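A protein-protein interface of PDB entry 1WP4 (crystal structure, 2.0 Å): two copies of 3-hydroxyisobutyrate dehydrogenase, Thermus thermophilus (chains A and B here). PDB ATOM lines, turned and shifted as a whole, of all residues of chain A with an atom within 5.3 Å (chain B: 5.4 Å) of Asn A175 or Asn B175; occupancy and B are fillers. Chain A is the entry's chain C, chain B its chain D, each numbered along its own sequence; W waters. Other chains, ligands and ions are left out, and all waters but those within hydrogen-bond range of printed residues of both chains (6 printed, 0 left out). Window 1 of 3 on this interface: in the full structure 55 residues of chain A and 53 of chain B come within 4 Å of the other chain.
Leu A172 touches Gly B205, and with the chains exchanged Gly A205 touches Leu B172.
Val A174 touches Ala B178, and with the chains exchanged Ala A178 touches Val B174.
Asn A175 touches Gly B205, and with the chains exchanged Gly A205 touches Asn B175.
Ser B207 touches its own counterpart, Ser A207.
16 positions are printed for both chains.
Of the 23 pairs that touch across the chains among the printed residues, 23 have their exchanged pair printed and touching as well.
Among the printed residues, merely in contact across the chains: Val A174 with Val B174 (3.3 Å), Leu A172 with Ser B204 (3.4 Å), Leu A171 with Ala B178 (3.5 Å), Ala A178 with Leu B171 (3.5 Å), Ser A204 with Leu B172 (3.5 Å), Gly A205 with Asn B175 (3.5 Å), Arg A206 with Ser B207 (3.6 Å), Leu A171 with Ala B179 (3.6 Å), Ser A207 with Ser B207 (3.7 Å), Ala A179 with Leu B171 (3.7 Å), Ser A207 with Arg B206 (3.7 Å), Leu A172 with Gly B205 (3.8 Å), Val A174 with Ala B178 (3.8 Å), Leu A171 with Gly B205 (3.8 Å), Asn A175 with Ser B207 (3.8 Å), Gly A205 with Leu B172 (3.9 Å), Ser A207 with Asn B175 (3.9 Å), Asn A175 with Arg B206 (3.9 Å), Gly A205 with Leu B171 (3.9 Å), Ala A178 with Val B174 (3.9 Å) and Arg A206 with Asn B175 (3.96 Å).
Printed residues of chain B within 4 Å of Leu A172: Ser B204 (3.4 Å) and Gly B205 (3.8 Å).
Asn A175 touches four residues of chain B.
Trp A177 touches none of the printed residues of chain B.
Printed residues of chain B within 4 Å of Ala A178: Leu B171 and Val B174.
Of the printed residues of chain B, Arg A206 touches Asn B175 and Ser B207.
Of the printed residues of chain A, Leu B171 touches Ala A178 (3.5 Å), Ala A179 (3.7 Å) and Gly A205 (3.9 Å).
Printed residues of chain A within 4 Å of Leu B172: Ser A204 (3.5 Å) and Gly A205 (3.9 Å).
Asn B175 touches four residues of chain A.
The nearest printed residue of chain B that does not touch Asn A175 is Ala B178 (5.2 Å).
The nearest residue of chain A that does not touch Asn B175 is Val A174 (5.2 Å).
O of Leu A171 sits close to OD1 of Asn A175 (3.1 Å).
The backbone NH of Ala A209 lies close to the side-chain hydroxyl of Ser A207 (3.3 Å).
The side-chain amide oxygen (OD1) of Asn B175 sits close to the backbone carbonyl oxygen (O) of Leu B171, at 3.1 Å.
The side-chain hydroxyl (OG) of Ser B207 sits close to the backbone NH (N) of Ala B209 (3.3 Å).
The side-chain amide oxygen (OD1) of Asn B175 lies close to the side-chain amide oxygen (OD1) of Asn A175.
The backbone carbonyl oxygen (O) of Gly B205 sits at hydrogen-bond distance from the side-chain amide nitrogen (ND2) of Asn A175 (3.5 Å).
Printed residues of chain A that touch a printed residue of chain B: Leu A171, Leu A172, Val A174, Asn A175, Ala A178, Ala A179, Ser A204, Gly A205, Arg A206 and Ser A207.
Hydrophobic or aromatic side chains of chain A that line the printed part of chain B: Leu A171, Leu A172, Val A174 and Ala A178.
Printed residues of chain B that touch a printed residue of chain A: Leu B171, Leu B172, Val B174, Asn B175, Ala B178, Ala B179, Ser B204, Gly B205, Arg B206 and Ser B207.
Hydrophobic or aromatic side chains of chain B that line the printed part of chain A: Leu B171, Leu B172, Val B174 and Ala B178.
Among the printed residues, no Asp or Glu carboxylate lies within 4 Å of a Lys or Arg side-chain nitrogen of the other chain.
Water W3 lies within hydrogen-bond range of OG of Ser B207 (2.7 Å), O of Gly B205 (2.8 Å) and ND2 of Asn A175 (3.2 Å).
Water W5 lies within hydrogen-bond range of OG of Ser A207 (2.7 Å), O of Gly A205 (2.7 Å) and ND2 of Asn B175 (3.1 Å).
Water W2 lies within hydrogen-bond range of the backbone carbonyl oxygen (O) of Ser B204 (2.7 Å), the backbone carbonyl oxygen (O) of Arg B206 (2.8 Å), the side-chain amide nitrogen (ND2) of Asn A175 (3.1 Å) and the backbone NH (N) of Ala A209 (3.4 Å).
Water W6 bridges OD1 of Asn B175 and O of Asn A175.
Water W4 lies within hydrogen-bond range of O of Arg A206 (2.8 Å), O of Ser A204 (2.8 Å), ND2 of Asn B175 (3.0 Å) and N of Ala B209 (3.5 Å).
Water W1 lies within hydrogen-bond range of O of Asn B175 (2.9 Å) and OD1 of Asn A175 (2.9 Å).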
ATOM      1  N   ALA A 170      21.535 -20.723  -8.000  1.00  0.00           N
ATOM      2  CA  ALA A 170      22.342 -19.578  -8.415  1.00  0.00           C
ATOM      3  C   ALA A 170      21.683 -18.312  -7.857  1.00  0.00           C
ATOM      4  O   ALA A 170      22.369 -17.348  -7.499  1.00  0.00           O
ATOM      5  CB  ALA A 170      22.436 -19.510  -9.940  1.00  0.00           C
ATOM      6  N   LEU A 171      20.351 -18.320  -7.775  1.00  0.00           N
ATOM      7  CA  LEU A 171      19.619 -17.173  -7.242  1.00  0.00           C
ATOM      8  C   LEU A 171      19.888 -17.067  -5.746  1.00  0.00           C
ATOM      9  O   LEU A 171      20.080 -15.976  -5.218  1.00  0.00           O
ATOM     10  CB  LEU A 171      18.111 -17.314  -7.498  1.00  0.00           C
ATOM     11  CG  LEU A 171      17.672 -17.310  -8.968  1.00  0.00           C
ATOM     12  CD1 LEU A 171      16.151 -17.265  -9.034  1.00  0.00           C
ATOM     13  CD2 LEU A 171      18.261 -16.103  -9.701  1.00  0.00           C
ATOM     14  N   LEU A 172      19.890 -18.205  -5.064  1.00  0.00           N
ATOM     15  CA  LEU A 172      20.176 -18.219  -3.636  1.00  0.00           C
ATOM     16  C   LEU A 172      21.581 -17.638  -3.432  1.00  0.00           C
ATOM     17  O   LEU A 172      21.784 -16.759  -2.599  1.00  0.00           O
ATOM     18  CB  LEU A 172      20.101 -19.655  -3.103  1.00  0.00           C
ATOM     19  CG  LEU A 172      20.522 -20.012  -1.667  1.00  0.00           C
ATOM     20  CD1 LEU A 172      22.032 -20.026  -1.562  1.00  0.00           C
ATOM     21  CD2 LEU A 172      19.912 -19.042  -0.676  1.00  0.00           C
ATOM     22  N   ALA A 173      22.539 -18.125  -4.215  1.00  0.00           N
ATOM     23  CA  ALA A 173      23.926 -17.667  -4.123  1.00  0.00           C
ATOM     24  C   ALA A 173      24.037 -16.153  -4.298  1.00  0.00           C
ATOM     25  O   ALA A 173      24.667 -15.474  -3.493  1.00  0.00           O
ATOM     26  CB  ALA A 173      24.770 -18.371  -5.170  1.00  0.00           C
ATOM     27  N   VAL A 174      23.427 -15.630  -5.360  1.00  0.00           N
ATOM     28  CA  VAL A 174      23.470 -14.192  -5.621  1.00  0.00           C
ATOM     29  C   VAL A 174      22.807 -13.378  -4.513  1.00  0.00           C
ATOM     30  O   VAL A 174      23.363 -12.380  -4.056  1.00  0.00           O
ATOM     31  CB  VAL A 174      22.786 -13.842  -6.968  1.00  0.00           C
ATOM     32  CG1 VAL A 174      22.680 -12.330  -7.129  1.00  0.00           C
ATOM     33  CG2 VAL A 174      23.587 -14.415  -8.109  1.00  0.00           C
ATOM     34  N   ASN A 175      21.617 -13.800  -4.089  1.00  0.00           N
ATOM     35  CA  ASN A 175      20.883 -13.097  -3.037  1.00  0.00           C
ATOM     36  C   ASN A 175      21.702 -13.036  -1.750  1.00  0.00           C
ATOM     37  O   ASN A 175      21.790 -11.994  -1.093  1.00  0.00           O
ATOM     38  CB  ASN A 175      19.556 -13.807  -2.733  1.00  0.00           C
ATOM     39  CG  ASN A 175      18.591 -13.796  -3.909  1.00  0.00           C
ATOM     40  OD1 ASN A 175      18.848 -13.176  -4.941  1.00  0.00           O
ATOM     41  ND2 ASN A 175      17.463 -14.491  -3.751  1.00  0.00           N
ATOM     42  N   LEU A 176      22.286 -14.175  -1.399  1.00  0.00           N
ATOM     43  CA  LEU A 176      23.090 -14.305  -0.194  1.00  0.00           C
ATOM     44  C   LEU A 176      24.339 -13.429  -0.205  1.00  0.00           C
ATOM     45  O   LEU A 176      24.608 -12.710   0.761  1.00  0.00           O
ATOM     46  CB  LEU A 176      23.490 -15.771  -0.018  1.00  0.00           C
ATOM     47  CG  LEU A 176      24.335 -16.178   1.193  1.00  0.00           C
ATOM     48  CD1 LEU A 176      23.581 -15.901   2.490  1.00  0.00           C
ATOM     49  CD2 LEU A 176      24.653 -17.661   1.079  1.00  0.00           C
ATOM     50  N   TRP A 177      25.101 -13.490  -1.295  1.00  0.00           N
ATOM     51  CA  TRP A 177      26.331 -12.714  -1.406  1.00  0.00           C
ATOM     52  C   TRP A 177      26.082 -11.208  -1.438  1.00  0.00           C
ATOM     53  O   TRP A 177      26.798 -10.442  -0.792  1.00  0.00           O
ATOM     54  CB  TRP A 177      27.119 -13.148  -2.648  1.00  0.00           C
ATOM     55  CG  TRP A 177      28.438 -12.458  -2.793  1.00  0.00           C
ATOM     56  CD1 TRP A 177      28.668 -11.240  -3.366  1.00  0.00           C
ATOM     57  CD2 TRP A 177      29.707 -12.925  -2.317  1.00  0.00           C
ATOM     58  NE1 TRP A 177      30.002 -10.919  -3.274  1.00  0.00           N
ATOM     59  CE2 TRP A 177      30.662 -11.936  -2.635  1.00  0.00           C
ATOM     60  CE3 TRP A 177      30.129 -14.086  -1.650  1.00  0.00           C
ATOM     61  CZ2 TRP A 177      32.020 -12.067  -2.308  1.00  0.00           C
ATOM     62  CZ3 TRP A 177      31.482 -14.217  -1.325  1.00  0.00           C
ATOM     63  CH2 TRP A 177      32.408 -13.213  -1.656  1.00  0.00           C
ATOM     64  N   ALA A 178      25.070 -10.781  -2.188  1.00  0.00           N
ATOM     65  CA  ALA A 178      24.753  -9.361  -2.265  1.00  0.00           C
ATOM     66  C   ALA A 178      24.353  -8.845  -0.882  1.00  0.00           C
ATOM     67  O   ALA A 178      24.738  -7.745  -0.485  1.00  0.00           O
ATOM     68  CB  ALA A 178      23.625  -9.125  -3.263  1.00  0.00           C
ATOM     69  N   ALA A 179      23.577  -9.641  -0.153  1.00  0.00           N
ATOM     70  CA  ALA A 179      23.142  -9.251   1.182  1.00  0.00           C
ATOM     71  C   ALA A 179      24.378  -9.131   2.070  1.00  0.00           C
ATOM     72  O   ALA A 179      24.459  -8.254   2.932  1.00  0.00           O
ATOM     73  CB  ALA A 179      22.178 -10.288   1.750  1.00  0.00           C
ATOM     74  N   GLY A 180      25.342 -10.017   1.848  1.00  0.00           N
ATOM     75  CA  GLY A 180      26.567  -9.976   2.622  1.00  0.00           C
ATOM     76  C   GLY A 180      27.346  -8.699   2.351  1.00  0.00           C
ATOM     77  O   GLY A 180      27.857  -8.075   3.280  1.00  0.00           O
ATOM     78  N   SER A 204      11.140  -4.692   0.437  1.00  0.00           N
ATOM     79  CA  SER A 204      11.290  -5.247  -0.899  1.00  0.00           C
ATOM     80  C   SER A 204      12.570  -6.039  -1.177  1.00  0.00           C
ATOM     81  O   SER A 204      12.611  -6.835  -2.114  1.00  0.00           O
ATOM     82  CB  SER A 204      11.163  -4.124  -1.933  1.00  0.00           C
ATOM     83  OG  SER A 204      12.235  -3.202  -1.808  1.00  0.00           O
ATOM     84  N   GLY A 205      13.609  -5.825  -0.379  1.00  0.00           N
ATOM     85  CA  GLY A 205      14.861  -6.528  -0.610  1.00  0.00           C
ATOM     86  C   GLY A 205      14.992  -7.854   0.115  1.00  0.00           C
ATOM     87  O   GLY A 205      16.061  -8.466   0.114  1.00  0.00           O
ATOM     88  N   ARG A 206      13.906  -8.314   0.724  1.00  0.00           N
ATOM     89  CA  ARG A 206      13.937  -9.570   1.455  1.00  0.00           C
ATOM     90  C   ARG A 206      14.047 -10.788   0.552  1.00  0.00           C
ATOM     91  O   ARG A 206      13.582 -10.794  -0.591  1.00  0.00           O
ATOM     92  CB  ARG A 206      12.694  -9.718   2.334  1.00  0.00           C
ATOM     93  CG  ARG A 206      11.380  -9.805   1.568  1.00  0.00           C
ATOM     94  CD  ARG A 206      10.255 -10.267   2.492  1.00  0.00           C
ATOM     95  NE  ARG A 206       8.955 -10.310   1.825  1.00  0.00           N
ATOM     96  CZ  ARG A 206       8.274  -9.233   1.437  1.00  0.00           C
ATOM     97  NH1 ARG A 206       8.766  -8.019   1.646  1.00  0.00           N
ATOM     98  NH2 ARG A 206       7.091  -9.372   0.850  1.00  0.00           N
ATOM     99  N   SER A 207      14.673 -11.826   1.087  1.00  0.00           N
ATOM    100  CA  SER A 207      14.842 -13.080   0.372  1.00  0.00           C
ATOM    101  C   SER A 207      14.976 -14.171   1.424  1.00  0.00           C
ATOM    102  O   SER A 207      15.123 -13.877   2.610  1.00  0.00           O
ATOM    103  CB  SER A 207      16.106 -13.045  -0.488  1.00  0.00           C
ATOM    104  OG  SER A 207      17.270 -12.910   0.314  1.00  0.00           O
ATOM    105  N   ALA A 209      17.381 -15.864   1.815  1.00  0.00           N
ATOM    106  CA  ALA A 209      18.729 -15.646   2.326  1.00  0.00           C
ATOM    107  C   ALA A 209      18.748 -14.718   3.542  1.00  0.00           C
ATOM    108  O   ALA A 209      19.357 -15.042   4.563  1.00  0.00           O
ATOM    109  CB  ALA A 209      19.624 -15.087   1.217  1.00  0.00           C
ATOM    110  N   ALA B 170      19.024  -1.756  -3.131  1.00  0.00           N
ATOM    111  CA  ALA B 170      20.108  -2.325  -3.920  1.00  0.00           C
ATOM    112  C   ALA B 170      19.938  -3.843  -3.932  1.00  0.00           C
ATOM    113  O   ALA B 170      20.203  -4.496  -4.942  1.00  0.00           O
ATOM    114  CB  ALA B 170      21.455  -1.951  -3.322  1.00  0.00           C
ATOM    115  N   LEU B 171      19.500  -4.403  -2.806  1.00  0.00           N
ATOM    116  CA  LEU B 171      19.292  -5.845  -2.724  1.00  0.00           C
ATOM    117  C   LEU B 171      18.117  -6.218  -3.620  1.00  0.00           C
ATOM    118  O   LEU B 171      18.151  -7.232  -4.312  1.00  0.00           O
ATOM    119  CB  LEU B 171      19.018  -6.277  -1.279  1.00  0.00           C
ATOM    120  CG  LEU B 171      20.172  -6.078  -0.286  1.00  0.00           C
ATOM    121  CD1 LEU B 171      19.808  -6.721   1.054  1.00  0.00           C
ATOM    122  CD2 LEU B 171      21.446  -6.705  -0.841  1.00  0.00           C
ATOM    123  N   LEU B 172      17.078  -5.389  -3.600  1.00  0.00           N
ATOM    124  CA  LEU B 172      15.916  -5.619  -4.447  1.00  0.00           C
ATOM    125  C   LEU B 172      16.388  -5.670  -5.894  1.00  0.00           C
ATOM    126  O   LEU B 172      16.044  -6.585  -6.640  1.00  0.00           O
ATOM    127  CB  LEU B 172      14.914  -4.475  -4.296  1.00  0.00           C
ATOM    128  CG  LEU B 172      13.882  -4.390  -5.426  1.00  0.00           C
ATOM    129  CD1 LEU B 172      12.979  -5.618  -5.366  1.00  0.00           C
ATOM    130  CD2 LEU B 172      13.063  -3.106  -5.299  1.00  0.00           C
ATOM    131  N   ALA B 173      17.187  -4.677  -6.276  1.00  0.00           N
ATOM    132  CA  ALA B 173      17.715  -4.579  -7.635  1.00  0.00           C
ATOM    133  C   ALA B 173      18.455  -5.840  -8.074  1.00  0.00           C
ATOM    134  O   ALA B 173      18.208  -6.374  -9.160  1.00  0.00           O
ATOM    135  CB  ALA B 173      18.646  -3.359  -7.748  1.00  0.00           C
ATOM    136  N   VAL B 174      19.377  -6.308  -7.238  1.00  0.00           N
ATOM    137  CA  VAL B 174      20.142  -7.505  -7.559  1.00  0.00           C
ATOM    138  C   VAL B 174      19.252  -8.733  -7.672  1.00  0.00           C
ATOM    139  O   VAL B 174      19.323  -9.470  -8.654  1.00  0.00           O
ATOM    140  CB  VAL B 174      21.207  -7.805  -6.488  1.00  0.00           C
ATOM    141  CG1 VAL B 174      21.851  -9.147  -6.775  1.00  0.00           C
ATOM    142  CG2 VAL B 174      22.252  -6.717  -6.475  1.00  0.00           C
ATOM    143  N   ASN B 175      18.437  -8.960  -6.648  1.00  0.00           N
ATOM    144  CA  ASN B 175      17.540 -10.112  -6.619  1.00  0.00           C
ATOM    145  C   ASN B 175      16.675 -10.163  -7.875  1.00  0.00           C
ATOM    146  O   ASN B 175      16.564 -11.203  -8.521  1.00  0.00           O
ATOM    147  CB  ASN B 175      16.631 -10.054  -5.383  1.00  0.00           C
ATOM    148  CG  ASN B 175      17.402 -10.164  -4.071  1.00  0.00           C
ATOM    149  OD1 ASN B 175      18.624 -10.315  -4.059  1.00  0.00           O
ATOM    150  ND2 ASN B 175      16.680 -10.086  -2.958  1.00  0.00           N
ATOM    151  N   LEU B 176      16.074  -9.027  -8.212  1.00  0.00           N
ATOM    152  CA  LEU B 176      15.206  -8.919  -9.380  1.00  0.00           C
ATOM    153  C   LEU B 176      15.930  -9.170 -10.703  1.00  0.00           C
ATOM    154  O   LEU B 176      15.444  -9.916 -11.547  1.00  0.00           O
ATOM    155  CB  LEU B 176      14.558  -7.531  -9.409  1.00  0.00           C
ATOM    156  CG  LEU B 176      13.607  -7.229 -10.566  1.00  0.00           C
ATOM    157  CD1 LEU B 176      12.409  -8.175 -10.512  1.00  0.00           C
ATOM    158  CD2 LEU B 176      13.157  -5.773 -10.471  1.00  0.00           C
ATOM    159  N   TRP B 177      17.090  -8.547 -10.889  1.00  0.00           N
ATOM    160  CA  TRP B 177      17.839  -8.724 -12.128  1.00  0.00           C
ATOM    161  C   TRP B 177      18.360 -10.152 -12.298  1.00  0.00           C
ATOM    162  O   TRP B 177      18.238 -10.735 -13.377  1.00  0.00           O
ATOM    163  CB  TRP B 177      19.000  -7.724 -12.197  1.00  0.00           C
ATOM    164  CG  TRP B 177      19.777  -7.807 -13.477  1.00  0.00           C
ATOM    165  CD1 TRP B 177      20.767  -8.702 -13.783  1.00  0.00           C
ATOM    166  CD2 TRP B 177      19.610  -6.984 -14.639  1.00  0.00           C
ATOM    167  NE1 TRP B 177      21.224  -8.484 -15.061  1.00  0.00           N
ATOM    168  CE2 TRP B 177      20.531  -7.436 -15.608  1.00  0.00           C
ATOM    169  CE3 TRP B 177      18.769  -5.908 -14.952  1.00  0.00           C
ATOM    170  CZ2 TRP B 177      20.637  -6.847 -16.875  1.00  0.00           C
ATOM    171  CZ3 TRP B 177      18.873  -5.323 -16.213  1.00  0.00           C
ATOM    172  CH2 TRP B 177      19.802  -5.796 -17.157  1.00  0.00           C
ATOM    173  N   ALA B 178      18.931 -10.716 -11.235  1.00  0.00           N
ATOM    174  CA  ALA B 178      19.453 -12.082 -11.290  1.00  0.00           C
ATOM    175  C   ALA B 178      18.327 -13.059 -11.614  1.00  0.00           C
ATOM    176  O   ALA B 178      18.503 -13.977 -12.411  1.00  0.00           O
ATOM    177  CB  ALA B 178      20.105 -12.453  -9.966  1.00  0.00           C
ATOM    178  N   ALA B 179      17.169 -12.866 -10.992  1.00  0.00           N
ATOM    179  CA  ALA B 179      16.032 -13.735 -11.262  1.00  0.00           C
ATOM    180  C   ALA B 179      15.688 -13.629 -12.750  1.00  0.00           C
ATOM    181  O   ALA B 179      15.339 -14.617 -13.392  1.00  0.00           O
ATOM    182  CB  ALA B 179      14.839 -13.322 -10.401  1.00  0.00           C
ATOM    183  N   GLY B 180      15.809 -12.420 -13.293  1.00  0.00           N
ATOM    184  CA  GLY B 180      15.527 -12.207 -14.702  1.00  0.00           C
ATOM    185  C   GLY B 180      16.473 -13.012 -15.569  1.00  0.00           C
ATOM    186  O   GLY B 180      16.046 -13.692 -16.505  1.00  0.00           O
ATOM    187  N   SER B 204      14.977 -22.414  -1.987  1.00  0.00           N
ATOM    188  CA  SER B 204      15.951 -21.492  -1.417  1.00  0.00           C
ATOM    189  C   SER B 204      16.249 -20.229  -2.224  1.00  0.00           C
ATOM    190  O   SER B 204      16.714 -19.238  -1.666  1.00  0.00           O
ATOM    191  CB  SER B 204      17.267 -22.233  -1.141  1.00  0.00           C
ATOM    192  OG  SER B 204      17.855 -22.684  -2.350  1.00  0.00           O
ATOM    193  N   GLY B 205      15.993 -20.261  -3.528  1.00  0.00           N
ATOM    194  CA  GLY B 205      16.261 -19.092  -4.350  1.00  0.00           C
ATOM    195  C   GLY B 205      15.182 -18.020  -4.288  1.00  0.00           C
ATOM    196  O   GLY B 205      15.322 -16.953  -4.889  1.00  0.00           O
ATOM    197  N   ARG B 206      14.114 -18.284  -3.545  1.00  0.00           N
ATOM    198  CA  ARG B 206      13.013 -17.329  -3.442  1.00  0.00           C
ATOM    199  C   ARG B 206      13.362 -15.978  -2.814  1.00  0.00           C
ATOM    200  O   ARG B 206      14.260 -15.868  -1.970  1.00  0.00           O
ATOM    201  CB  ARG B 206      11.843 -17.950  -2.676  1.00  0.00           C
ATOM    202  CG  ARG B 206      12.063 -18.171  -1.191  1.00  0.00           C
ATOM    203  CD  ARG B 206      10.732 -18.570  -0.541  1.00  0.00           C
ATOM    204  NE  ARG B 206      10.819 -18.820   0.898  1.00  0.00           N
ATOM    205  CZ  ARG B 206      11.463 -19.849   1.447  1.00  0.00           C
ATOM    206  NH1 ARG B 206      12.087 -20.732   0.679  1.00  0.00           N
ATOM    207  NH2 ARG B 206      11.467 -20.006   2.764  1.00  0.00           N
ATOM    208  N   SER B 207      12.633 -14.952  -3.246  1.00  0.00           N
ATOM    209  CA  SER B 207      12.801 -13.587  -2.756  1.00  0.00           C
ATOM    210  C   SER B 207      11.522 -12.822  -3.067  1.00  0.00           C
ATOM    211  O   SER B 207      10.675 -13.309  -3.814  1.00  0.00           O
ATOM    212  CB  SER B 207      13.968 -12.902  -3.464  1.00  0.00           C
ATOM    213  OG  SER B 207      13.685 -12.723  -4.845  1.00  0.00           O
ATOM    214  N   ALA B 209      11.207 -10.497  -4.945  1.00  0.00           N
ATOM    215  CA  ALA B 209      11.202 -10.307  -6.391  1.00  0.00           C
ATOM    216  C   ALA B 209      10.510 -11.458  -7.123  1.00  0.00           C
ATOM    217  O   ALA B 209       9.613 -11.225  -7.938  1.00  0.00           O
ATOM    218  CB  ALA B 209      12.627 -10.140  -6.905  1.00  0.00           C
HETATM  219  O   HOH W   1      17.340 -13.687  -7.355  1.00  0.00           O
HETATM  220  O   HOH W   2      16.956 -16.538  -1.522  1.00  0.00           O
HETATM  221  O   HOH W   3      15.296 -14.452  -6.047  1.00  0.00           O
HETATM  222  O   HOH W   4      13.778  -9.287  -2.924  1.00  0.00           O
HETATM  223  O   HOH W   5      17.898 -10.373  -0.176  1.00  0.00           O
HETATM  224  O   HOH W   6      20.114  -9.876  -1.786  1.00  0.00           O
